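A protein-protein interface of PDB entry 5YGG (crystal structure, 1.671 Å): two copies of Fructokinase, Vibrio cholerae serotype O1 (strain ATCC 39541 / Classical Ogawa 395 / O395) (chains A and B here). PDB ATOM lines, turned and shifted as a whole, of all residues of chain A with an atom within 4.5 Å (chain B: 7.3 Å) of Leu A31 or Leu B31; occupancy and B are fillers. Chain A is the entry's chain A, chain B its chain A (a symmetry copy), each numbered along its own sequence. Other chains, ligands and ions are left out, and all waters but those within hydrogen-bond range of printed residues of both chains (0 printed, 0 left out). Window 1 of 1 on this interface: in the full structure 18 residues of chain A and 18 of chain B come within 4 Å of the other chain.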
ATOM      1  N   VAL A  29     -27.310  -6.886  -8.634  1.00  0.00           N
ATOM      2  CA  VAL A  29     -26.542  -5.643  -8.617  1.00  0.00           C
ATOM      3  C   VAL A  29     -27.129  -4.738  -9.682  1.00  0.00           C
ATOM      4  O   VAL A  29     -27.180  -5.108 -10.866  1.00  0.00           O
ATOM      5  CB  VAL A  29     -25.045  -5.878  -8.871  1.00  0.00           C
ATOM      6  CG1 VAL A  29     -24.306  -4.540  -9.075  1.00  0.00           C
ATOM      7  CG2 VAL A  29     -24.455  -6.680  -7.722  1.00  0.00           C
ATOM      8  N   ASP A  30     -27.598  -3.574  -9.242  1.00  0.00           N
ATOM      9  CA  ASP A  30     -28.139  -2.535 -10.117  1.00  0.00           C
ATOM     10  C   ASP A  30     -27.051  -1.551 -10.485  1.00  0.00           C
ATOM     11  O   ASP A  30     -26.496  -0.909  -9.597  1.00  0.00           O
ATOM     12  CB  ASP A  30     -29.273  -1.752  -9.431  1.00  0.00           C
ATOM     13  CG  ASP A  30     -30.551  -2.542  -9.288  1.00  0.00           C
ATOM     14  OD1 ASP A  30     -30.827  -3.421 -10.133  1.00  0.00           O
ATOM     15  OD2 ASP A  30     -31.309  -2.264  -8.336  1.00  0.00           O
ATOM     16  N   LEU A  31     -26.750  -1.418 -11.777  1.00  0.00           N
ATOM     17  CA  LEU A  31     -25.758  -0.446 -12.221  1.00  0.00           C
ATOM     18  C   LEU A  31     -26.491   0.835 -12.571  1.00  0.00           C
ATOM     19  O   LEU A  31     -27.233   0.884 -13.545  1.00  0.00           O
ATOM     20  CB  LEU A  31     -24.965  -0.970 -13.418  1.00  0.00           C
ATOM     21  CG  LEU A  31     -24.176  -2.246 -13.086  1.00  0.00           C
ATOM     22  CD1 LEU A  31     -23.576  -2.863 -14.338  1.00  0.00           C
ATOM     23  CD2 LEU A  31     -23.082  -1.919 -12.070  1.00  0.00           C
ATOM     24  N   ILE A  32     -26.310   1.866 -11.750  1.00  0.00           N
ATOM     25  CA  ILE A  32     -27.068   3.098 -11.913  1.00  0.00           C
ATOM     26  C   ILE A  32     -26.141   4.230 -12.327  1.00  0.00           C
ATOM     27  O   ILE A  32     -25.158   4.508 -11.637  1.00  0.00           O
ATOM     28  CB  ILE A  32     -27.822   3.466 -10.598  1.00  0.00           C
ATOM     29  CG1 ILE A  32     -28.662   2.269 -10.126  1.00  0.00           C
ATOM     30  CG2 ILE A  32     -28.677   4.691 -10.800  1.00  0.00           C
ATOM     31  CD1 ILE A  32     -29.513   2.557  -8.887  1.00  0.00           C
ATOM     32  N   PRO A  33     -26.431   4.874 -13.474  1.00  0.00           N
ATOM     33  CA  PRO A  33     -25.609   5.981 -13.962  1.00  0.00           C
ATOM     34  C   PRO A  33     -25.386   7.028 -12.876  1.00  0.00           C
ATOM     35  O   PRO A  33     -26.348   7.439 -12.230  1.00  0.00           O
ATOM     36  CB  PRO A  33     -26.444   6.548 -15.119  1.00  0.00           C
ATOM     37  CG  PRO A  33     -27.189   5.360 -15.637  1.00  0.00           C
ATOM     38  CD  PRO A  33     -27.557   4.589 -14.386  1.00  0.00           C
ATOM     39  N   TYR A  39     -20.936   4.056 -13.355  1.00  0.00           N
ATOM     40  CA  TYR A  39     -22.117   3.485 -12.714  1.00  0.00           C
ATOM     41  C   TYR A  39     -21.885   3.415 -11.218  1.00  0.00           C
ATOM     42  O   TYR A  39     -20.780   3.098 -10.779  1.00  0.00           O
ATOM     43  CB  TYR A  39     -22.410   2.079 -13.227  1.00  0.00           C
ATOM     44  CG  TYR A  39     -22.918   1.986 -14.631  1.00  0.00           C
ATOM     45  CD1 TYR A  39     -24.182   2.451 -14.972  1.00  0.00           C
ATOM     46  CD2 TYR A  39     -22.144   1.394 -15.621  1.00  0.00           C
ATOM     47  CE1 TYR A  39     -24.657   2.340 -16.271  1.00  0.00           C
ATOM     48  CE2 TYR A  39     -22.603   1.278 -16.913  1.00  0.00           C
ATOM     49  CZ  TYR A  39     -23.858   1.744 -17.236  1.00  0.00           C
ATOM     50  OH  TYR A  39     -24.286   1.621 -18.537  1.00  0.00           O
ATOM     51  N   LEU A  40     -22.914   3.730 -10.444  1.00  0.00           N
ATOM     52  CA  LEU A  40     -22.964   3.352  -9.039  1.00  0.00           C
ATOM     53  C   LEU A  40     -23.201   1.862  -8.946  1.00  0.00           C
ATOM     54  O   LEU A  40     -24.072   1.347  -9.642  1.00  0.00           O
ATOM     55  CB  LEU A  40     -24.100   4.064  -8.320  1.00  0.00           C
ATOM     56  CG  LEU A  40     -23.860   5.251  -7.409  1.00  0.00           C
ATOM     57  CD1 LEU A  40     -25.206   5.733  -6.880  1.00  0.00           C
ATOM     58  CD2 LEU A  40     -22.935   4.862  -6.263  1.00  0.00           C
ATOM     59  N   THR A 100     -27.374  -9.074 -13.057  1.00  0.00           N
ATOM     60  CA  THR A 100     -26.784  -7.753 -13.208  1.00  0.00           C
ATOM     61  C   THR A 100     -27.699  -6.895 -14.057  1.00  0.00           C
ATOM     62  O   THR A 100     -28.020  -7.257 -15.188  1.00  0.00           O
ATOM     63  CB  THR A 100     -25.395  -7.834 -13.857  1.00  0.00           C
ATOM     64  OG1 THR A 100     -24.565  -8.700 -13.074  1.00  0.00           O
ATOM     65  CG2 THR A 100     -24.762  -6.446 -13.945  1.00  0.00           C
ATOM     66  N   VAL A 101     -28.112  -5.757 -13.513  1.00  0.00           N
ATOM     67  CA  VAL A 101     -29.127  -4.928 -14.156  1.00  0.00           C
ATOM     68  C   VAL A 101     -28.629  -3.513 -14.397  1.00  0.00           C
ATOM     69  O   VAL A 101     -28.075  -2.905 -13.492  1.00  0.00           O
ATOM     70  CB  VAL A 101     -30.390  -4.873 -13.289  1.00  0.00           C
ATOM     71  CG1 VAL A 101     -31.376  -3.866 -13.848  1.00  0.00           C
ATOM     72  CG2 VAL A 101     -31.004  -6.266 -13.194  1.00  0.00           C
ATOM     73  N   VAL A 102     -28.810  -2.998 -15.613  1.00  0.00           N
ATOM     74  CA  VAL A 102     -28.461  -1.611 -15.908  1.00  0.00           C
ATOM     75  C   VAL A 102     -29.709  -0.752 -15.815  1.00  0.00           C
ATOM     76  O   VAL A 102     -30.747  -1.088 -16.390  1.00  0.00           O
ATOM     77  CB  VAL A 102     -27.849  -1.443 -17.301  1.00  0.00           C
ATOM     78  CG1 VAL A 102     -27.427   0.021 -17.512  1.00  0.00           C
ATOM     79  CG2 VAL A 102     -26.665  -2.380 -17.478  1.00  0.00           C
ATOM     80  N   VAL A 103     -29.608   0.368 -15.110  1.00  0.00           N
ATOM     81  CA  VAL A 103     -30.772   1.221 -14.891  1.00  0.00           C
ATOM     82  C   VAL A 103     -30.754   2.448 -15.806  1.00  0.00           C
ATOM     83  O   VAL A 103     -29.704   3.045 -16.037  1.00  0.00           O
ATOM     84  CB  VAL A 103     -30.857   1.658 -13.411  1.00  0.00           C
ATOM     85  CG1 VAL A 103     -32.033   2.612 -13.183  1.00  0.00           C
ATOM     86  CG2 VAL A 103     -30.995   0.431 -12.507  1.00  0.00           C
ATOM     87  N   VAL B  28     -16.720  -6.067 -25.635  1.00  0.00           N
ATOM     88  CA  VAL B  28     -17.254  -6.210 -24.277  1.00  0.00           C
ATOM     89  C   VAL B  28     -17.204  -4.880 -23.543  1.00  0.00           C
ATOM     90  O   VAL B  28     -16.371  -4.030 -23.846  1.00  0.00           O
ATOM     91  CB  VAL B  28     -16.489  -7.288 -23.428  1.00  0.00           C
ATOM     92  CG1 VAL B  28     -16.046  -8.472 -24.283  1.00  0.00           C
ATOM     93  CG2 VAL B  28     -15.332  -6.692 -22.692  1.00  0.00           C
ATOM     94  N   VAL B  29     -18.101  -4.706 -22.581  1.00  0.00           N
ATOM     95  CA  VAL B  29     -18.017  -3.572 -21.664  1.00  0.00           C
ATOM     96  C   VAL B  29     -17.276  -4.047 -20.430  1.00  0.00           C
ATOM     97  O   VAL B  29     -17.702  -5.008 -19.769  1.00  0.00           O
ATOM     98  CB  VAL B  29     -19.401  -3.022 -21.286  1.00  0.00           C
ATOM     99  CG1 VAL B  29     -19.289  -1.986 -20.149  1.00  0.00           C
ATOM    100  CG2 VAL B  29     -20.069  -2.437 -22.520  1.00  0.00           C
ATOM    101  N   ASP B  30     -16.154  -3.388 -20.154  1.00  0.00           N
ATOM    102  CA  ASP B  30     -15.333  -3.647 -18.972  1.00  0.00           C
ATOM    103  C   ASP B  30     -15.733  -2.714 -17.850  1.00  0.00           C
ATOM    104  O   ASP B  30     -15.624  -1.501 -18.010  1.00  0.00           O
ATOM    105  CB  ASP B  30     -13.837  -3.422 -19.262  1.00  0.00           C
ATOM    106  CG  ASP B  30     -13.226  -4.491 -20.135  1.00  0.00           C
ATOM    107  OD1 ASP B  30     -13.682  -5.654 -20.092  1.00  0.00           O
ATOM    108  OD2 ASP B  30     -12.256  -4.175 -20.854  1.00  0.00           O
ATOM    109  N   LEU B  31     -16.184  -3.263 -16.722  1.00  0.00           N
ATOM    110  CA  LEU B  31     -16.531  -2.437 -15.572  1.00  0.00           C
ATOM    111  C   LEU B  31     -15.306  -2.345 -14.682  1.00  0.00           C
ATOM    112  O   LEU B  31     -14.899  -3.329 -14.075  1.00  0.00           O
ATOM    113  CB  LEU B  31     -17.721  -3.021 -14.809  1.00  0.00           C
ATOM    114  CG  LEU B  31     -18.992  -3.089 -15.670  1.00  0.00           C
ATOM    115  CD1 LEU B  31     -20.092  -3.865 -14.966  1.00  0.00           C
ATOM    116  CD2 LEU B  31     -19.461  -1.673 -16.001  1.00  0.00           C
ATOM    117  N   ILE B  32     -14.695  -1.165 -14.634  1.00  0.00           N
ATOM    118  CA  ILE B  32     -13.435  -0.999 -13.922  1.00  0.00           C
ATOM    119  C   ILE B  32     -13.635  -0.103 -12.711  1.00  0.00           C
ATOM    120  O   ILE B  32     -14.114   1.025 -12.848  1.00  0.00           O
ATOM    121  CB  ILE B  32     -12.338  -0.410 -14.860  1.00  0.00           C
ATOM    122  CG1 ILE B  32     -12.231  -1.259 -16.136  1.00  0.00           C
ATOM    123  CG2 ILE B  32     -11.014  -0.326 -14.145  1.00  0.00           C
ATOM    124  CD1 ILE B  32     -11.118  -0.814 -17.088  1.00  0.00           C
ATOM    125  N   PRO B  33     -13.295  -0.608 -11.509  1.00  0.00           N
ATOM    126  CA  PRO B  33     -13.441   0.172 -10.279  1.00  0.00           C
ATOM    127  C   PRO B  33     -12.796   1.547 -10.414  1.00  0.00           C
ATOM    128  O   PRO B  33     -11.655   1.635 -10.864  1.00  0.00           O
ATOM    129  CB  PRO B  33     -12.710  -0.686  -9.237  1.00  0.00           C
ATOM    130  CG  PRO B  33     -12.892  -2.085  -9.735  1.00  0.00           C
ATOM    131  CD  PRO B  33     -12.754  -1.955 -11.239  1.00  0.00           C
ATOM    132  N   ASP B  34     -13.532   2.599 -10.076  1.00  0.00           N
ATOM    133  CA  ASP B  34     -12.999   3.951 -10.133  1.00  0.00           C
ATOM    134  C   ASP B  34     -13.729   4.836  -9.136  1.00  0.00           C
ATOM    135  O   ASP B  34     -14.773   5.404  -9.447  1.00  0.00           O
ATOM    136  CB  ASP B  34     -13.107   4.527 -11.546  1.00  0.00           C
ATOM    137  CG  ASP B  34     -12.280   5.784 -11.725  1.00  0.00           C
ATOM    138  OD1 ASP B  34     -11.080   5.764 -11.384  1.00  0.00           O
ATOM    139  OD2 ASP B  34     -12.823   6.793 -12.208  1.00  0.00           O
ATOM    140  N   HIS B  38     -18.199   2.943  -7.372  1.00  0.00           N
ATOM    141  CA  HIS B  38     -18.411   3.222  -8.790  1.00  0.00           C
ATOM    142  C   HIS B  38     -17.578   2.349  -9.715  1.00  0.00           C
ATOM    143  O   HIS B  38     -16.465   1.946  -9.378  1.00  0.00           O
ATOM    144  CB  HIS B  38     -18.081   4.678  -9.118  1.00  0.00           C
ATOM    145  CG  HIS B  38     -18.975   5.670  -8.451  1.00  0.00           C
ATOM    146  ND1 HIS B  38     -19.971   6.349  -9.134  1.00  0.00           N
ATOM    147  CD2 HIS B  38     -19.042   6.093  -7.174  1.00  0.00           C
ATOM    148  CE1 HIS B  38     -20.591   7.152  -8.300  1.00  0.00           C
ATOM    149  NE2 HIS B  38     -20.055   7.022  -7.100  1.00  0.00           N
ATOM    150  N   TYR B  39     -18.120   2.080 -10.894  1.00  0.00           N
ATOM    151  CA  TYR B  39     -17.354   1.493 -11.989  1.00  0.00           C
ATOM    152  C   TYR B  39     -17.250   2.500 -13.117  1.00  0.00           C
ATOM    153  O   TYR B  39     -18.214   3.209 -13.402  1.00  0.00           O
ATOM    154  CB  TYR B  39     -18.019   0.229 -12.526  1.00  0.00           C
ATOM    155  CG  TYR B  39     -17.972  -0.967 -11.628  1.00  0.00           C
ATOM    156  CD1 TYR B  39     -16.777  -1.623 -11.362  1.00  0.00           C
ATOM    157  CD2 TYR B  39     -19.140  -1.472 -11.069  1.00  0.00           C
ATOM    158  CE1 TYR B  39     -16.744  -2.746 -10.549  1.00  0.00           C
ATOM    159  CE2 TYR B  39     -19.121  -2.585 -10.260  1.00  0.00           C
ATOM    160  CZ  TYR B  39     -17.928  -3.224 -10.005  1.00  0.00           C
ATOM    161  OH  TYR B  39     -17.940  -4.328  -9.186  1.00  0.00           O
ATOM    162  N   LEU B  40     -16.081   2.575 -13.738  1.00  0.00           N
ATOM    163  CA  LEU B  40     -15.944   3.197 -15.047  1.00  0.00           C
ATOM    164  C   LEU B  40     -16.567   2.288 -16.083  1.00  0.00           C
ATOM    165  O   LEU B  40     -16.311   1.088 -16.061  1.00  0.00           O
ATOM    166  CB  LEU B  40     -14.480   3.400 -15.406  1.00  0.00           C
ATOM    167  CG  LEU B  40     -13.809   4.756 -15.318  1.00  0.00           C
ATOM    168  CD1 LEU B  40     -12.347   4.597 -15.720  1.00  0.00           C
ATOM    169  CD2 LEU B  40     -14.514   5.757 -16.224  1.00  0.00           C
ATOM    170  N   LYS B  41     -17.364   2.841 -16.994  1.00  0.00           N
ATOM    171  CA  LYS B  41     -17.905   2.042 -18.097  1.00  0.00           C
ATOM    172  C   LYS B  41     -16.968   2.143 -19.295  1.00  0.00           C
ATOM    173  O   LYS B  41     -17.025   3.117 -20.048  1.00  0.00           O
ATOM    174  CB  LYS B  41     -19.303   2.536 -18.464  1.00  0.00           C
ATOM    175  CG  LYS B  41     -19.957   1.845 -19.662  1.00  0.00           C
ATOM    176  CD  LYS B  41     -21.060   2.742 -20.164  1.00  0.00           C
ATOM    177  CE  LYS B  41     -21.939   2.083 -21.191  1.00  0.00           C
ATOM    178  NZ  LYS B  41     -23.063   3.001 -21.544  1.00  0.00           N
ATOM    179  N   CYS B  42     -16.105   1.144 -19.467  1.00  0.00           N
ATOM    180  CA  CYS B  42     -15.049   1.193 -20.468  1.00  0.00           C
ATOM    181  C   CYS B  42     -15.289   0.252 -21.622  1.00  0.00           C
ATOM    182  O   CYS B  42     -15.571  -0.926 -21.417  1.00  0.00           O
ATOM    183  CB  CYS B  42     -13.697   0.844 -19.834  1.00  0.00           C
ATOM    184  SG  CYS B  42     -13.169   2.010 -18.559  1.00  0.00           S
ATOM    185  N   PHE B  72     -25.376  -1.920 -24.137  1.00  0.00           N
ATOM    186  CA  PHE B  72     -23.939  -2.206 -24.179  1.00  0.00           C
ATOM    187  C   PHE B  72     -23.476  -2.547 -25.601  1.00  0.00           C
ATOM    188  O   PHE B  72     -22.381  -2.148 -26.025  1.00  0.00           O
ATOM    189  CB  PHE B  72     -23.577  -3.346 -23.220  1.00  0.00           C
ATOM    190  CG  PHE B  72     -23.489  -2.919 -21.771  1.00  0.00           C
ATOM    191  CD1 PHE B  72     -23.835  -1.633 -21.389  1.00  0.00           C
ATOM    192  CD2 PHE B  72     -23.051  -3.809 -20.796  1.00  0.00           C
ATOM    193  CE1 PHE B  72     -23.762  -1.236 -20.057  1.00  0.00           C
ATOM    194  CE2 PHE B  72     -22.980  -3.421 -19.461  1.00  0.00           C
ATOM    195  CZ  PHE B  72     -23.331  -2.129 -19.093  1.00  0.00           C
ATOM    196  N   THR B 100     -20.245  -8.675 -20.578  1.00  0.00           N
ATOM    197  CA  THR B 100     -20.012  -7.699 -19.524  1.00  0.00           C
ATOM    198  C   THR B 100     -18.987  -8.251 -18.555  1.00  0.00           C
ATOM    199  O   THR B 100     -19.180  -9.325 -17.988  1.00  0.00           O
ATOM    200  CB  THR B 100     -21.310  -7.365 -18.776  1.00  0.00           C
ATOM    201  OG1 THR B 100     -22.285  -6.906 -19.718  1.00  0.00           O
ATOM    202  CG2 THR B 100     -21.060  -6.290 -17.720  1.00  0.00           C
ATOM    203  N   VAL B 101     -17.900  -7.513 -18.361  1.00  0.00           N
ATOM    204  CA  VAL B 101     -16.767  -8.010 -17.588  1.00  0.00           C
ATOM    205  C   VAL B 101     -16.427  -7.089 -16.428  1.00  0.00           C
ATOM    206  O   VAL B 101     -16.331  -5.885 -16.622  1.00  0.00           O
ATOM    207  CB  VAL B 101     -15.536  -8.154 -18.490  1.00  0.00           C
ATOM    208  CG1 VAL B 101     -14.307  -8.485 -17.665  1.00  0.00           C
ATOM    209  CG2 VAL B 101     -15.802  -9.218 -19.551  1.00  0.00           C
ATOM    210  N   VAL B 102     -16.262  -7.648 -15.230  1.00  0.00           N
ATOM    211  CA  VAL B 102     -15.830  -6.857 -14.080  1.00  0.00           C
ATOM    212  C   VAL B 102     -14.332  -7.018 -13.898  1.00  0.00           C
ATOM    213  O   VAL B 102     -13.816  -8.138 -13.896  1.00  0.00           O
ATOM    214  CB  VAL B 102     -16.532  -7.275 -12.785  1.00  0.00           C
ATOM    215  CG1 VAL B 102     -16.098  -6.350 -11.635  1.00  0.00           C
ATOM    216  CG2 VAL B 102     -18.041  -7.245 -12.964  1.00  0.00           C
ATOM    217  N   VAL B 103     -13.632  -5.904 -13.725  1.00  0.00           N
ATOM    218  CA  VAL B 103     -12.176  -5.943 -13.624  1.00  0.00           C
ATOM    219  C   VAL B 103     -11.706  -5.808 -12.174  1.00  0.00           C
ATOM    220  O   VAL B 103     -12.263  -5.029 -11.403  1.00  0.00           O
ATOM    221  CB  VAL B 103     -11.539  -4.840 -14.499  1.00  0.00           C
ATOM    222  CG1 VAL B 103     -10.016  -4.824 -14.346  1.00  0.00           C
ATOM    223  CG2 VAL B 103     -11.916  -5.048 -15.968  1.00  0.00           C
ATOM    224  N   ASP B 104     -10.703  -6.602 -11.806  1.00  0.00           N
ATOM    225  CA  ASP B 104     -10.053  -6.509 -10.498  1.00  0.00           C
ATOM    226  C   ASP B 104      -8.712  -5.815 -10.689  1.00  0.00           C
ATOM    227  O   ASP B 104      -7.826  -6.348 -11.354  1.00  0.00           O
ATOM    228  CB  ASP B 104      -9.863  -7.901  -9.887  1.00  0.00           C
ATOM    229  CG  ASP B 104      -9.306  -7.863  -8.473  1.00  0.00           C
ATOM    230  OD1 ASP B 104      -8.809  -6.803  -8.039  1.00  0.00           O
ATOM    231  OD2 ASP B 104      -9.358  -8.912  -7.794  1.00  0.00           O
ATOM    232  N   LEU B 105      -8.560  -4.628 -10.110  1.00  0.00           N
ATOM    233  CA  LEU B 105      -7.365  -3.827 -10.370  1.00  0.00           C
ATOM    234  C   LEU B 105      -6.140  -4.359  -9.622  1.00  0.00           C
ATOM    235  O   LEU B 105      -5.013  -3.946  -9.891  1.00  0.00           O
ATOM    236  CB  LEU B 105      -7.626  -2.361 -10.020  1.00  0.00           C
ATOM    237  CG  LEU B 105      -8.566  -1.696 -11.038  1.00  0.00           C
ATOM    238  CD1 LEU B 105      -9.071  -0.348 -10.543  1.00  0.00           C
ATOM    239  CD2 LEU B 105      -7.898  -1.557 -12.409  1.00  0.00           C
ATOM    240  N   SER B 112      -7.600 -11.073 -13.719  1.00  0.00           N
ATOM    241  CA  SER B 112      -8.274  -9.820 -13.377  1.00  0.00           C
ATOM    242  C   SER B 112      -9.735  -9.752 -13.849  1.00  0.00           C
ATOM    243  O   SER B 112     -10.463  -8.839 -13.470  1.00  0.00           O
ATOM    244  CB  SER B 112      -7.497  -8.629 -13.946  1.00  0.00           C
ATOM    245  OG  SER B 112      -7.622  -8.576 -15.354  1.00  0.00           O
ATOM    246  N   MET B 116     -19.512 -11.889 -16.648  1.00  0.00           N
ATOM    247  CA  MET B 116     -20.861 -11.968 -16.083  1.00  0.00           C
ATOM    248  C   MET B 116     -21.882 -12.533 -17.061  1.00  0.00           C
ATOM    249  O   MET B 116     -22.965 -12.973 -16.652  1.00  0.00           O
ATOM    250  CB  MET B 116     -21.327 -10.590 -15.604  1.00  0.00           C
ATOM    251  CG  MET B 116     -20.528 -10.052 -14.428  1.00  0.00           C
ATOM    252  SD  MET B 116     -20.520 -11.156 -13.001  1.00  0.00           S
ATOM    253  CE  MET B 116     -22.257 -11.115 -12.488  1.00  0.00           C
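Of the 11 printed residues of chain A, 5 touch a printed residue of chain B.
Hydrophobic or aromatic side chains of chain A that line the printed part of chain B: Leu A31, Tyr A39, Leu A40 and Val A102.
Of the 21 printed residues of chain B, 6 touch a printed residue of chain A.
Hydrophobic or aromatic side chains of chain B within 4 Å of the printed part of chain A: Leu B31, His B38, Phe B72 and Met B116.
Among the printed residues, no Asp or Glu carboxylate lies within 4 Å of a Lys or Arg side-chain nitrogen of the other chain.
Leu A31 touches just one residue of chain B: Leu B31 (3.7 Å).
Printed residues of chain A within 4 Å of Leu B31: Leu A31.
Printed residues of chain A within 4 Å of Lys B41: Tyr A39 (3.5 Å).
Of the printed residues of chain B, Leu A40 touches His B38.
Of the printed residues of chain A, His B38 touches Tyr A39 (3.1 Å) and Leu A40 (3.7 Å).
Pro A33 touches none of the printed residues of chain B.
The nearest residue of chain B that does not touch Leu A31 is Tyr B39 (4.1 Å).
The nearest residue of chain A that does not touch Leu B31 is Tyr A39 (4.1 Å).
The nearest printed residue of chain A that does not touch Phe B72 is Leu A31 (4.8 Å).
O of Tyr B39 sits at hydrogen-bond distance from N of Tyr A39 (2.9 Å).
Leu A31 touches its own counterpart, Leu B31.
Tyr B39 touches its own counterpart, Tyr A39.
Positions printed for both chains: 29, 30, 31, 32, 33, 39, 40, 100, 101, 102 and 103.
Of the 8 pairs that touch across the chains among the printed residues, 2 have their exchanged pair printed and touching as well.
CD1 of Leu A31 touches CD1 of Leu B31, 3.7 Å away.
His B38 touches Tyr A39 (CA to O, 3.1 Å).
Lys B41 touches Tyr A39 (NZ to OH, 3.5 Å).
OH of Tyr A39 touches CE1 of Phe B72, at 3.3 Å.
NE2 of His B38 touches CD2 of Leu A40, 3.7 Å away.
Thr A100 touches Met B116 (OG1 to CE, 3.4 Å).
Val A102 touches Phe B72.
The backbone carbonyl oxygen (O) of Val A101 lies within hydrogen-bond range of the backbone NH (N) of Leu A31 (2.6 Å).
N of Val A103 lies within hydrogen-bond range of O of Leu A31.
O of Ile A32 is in hydrogen-bond range of N of Leu A40.
The backbone NH (N) of Leu B31 is in hydrogen-bond range of the backbone carbonyl oxygen (O) of Val B101, 2.6 Å away.
N of Val B103 sits at hydrogen-bond distance from O of Leu B31.
The backbone carbonyl oxygen (O) of Thr B100 lies within hydrogen-bond range of the backbone NH (N) of Met B116 (2.9 Å).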
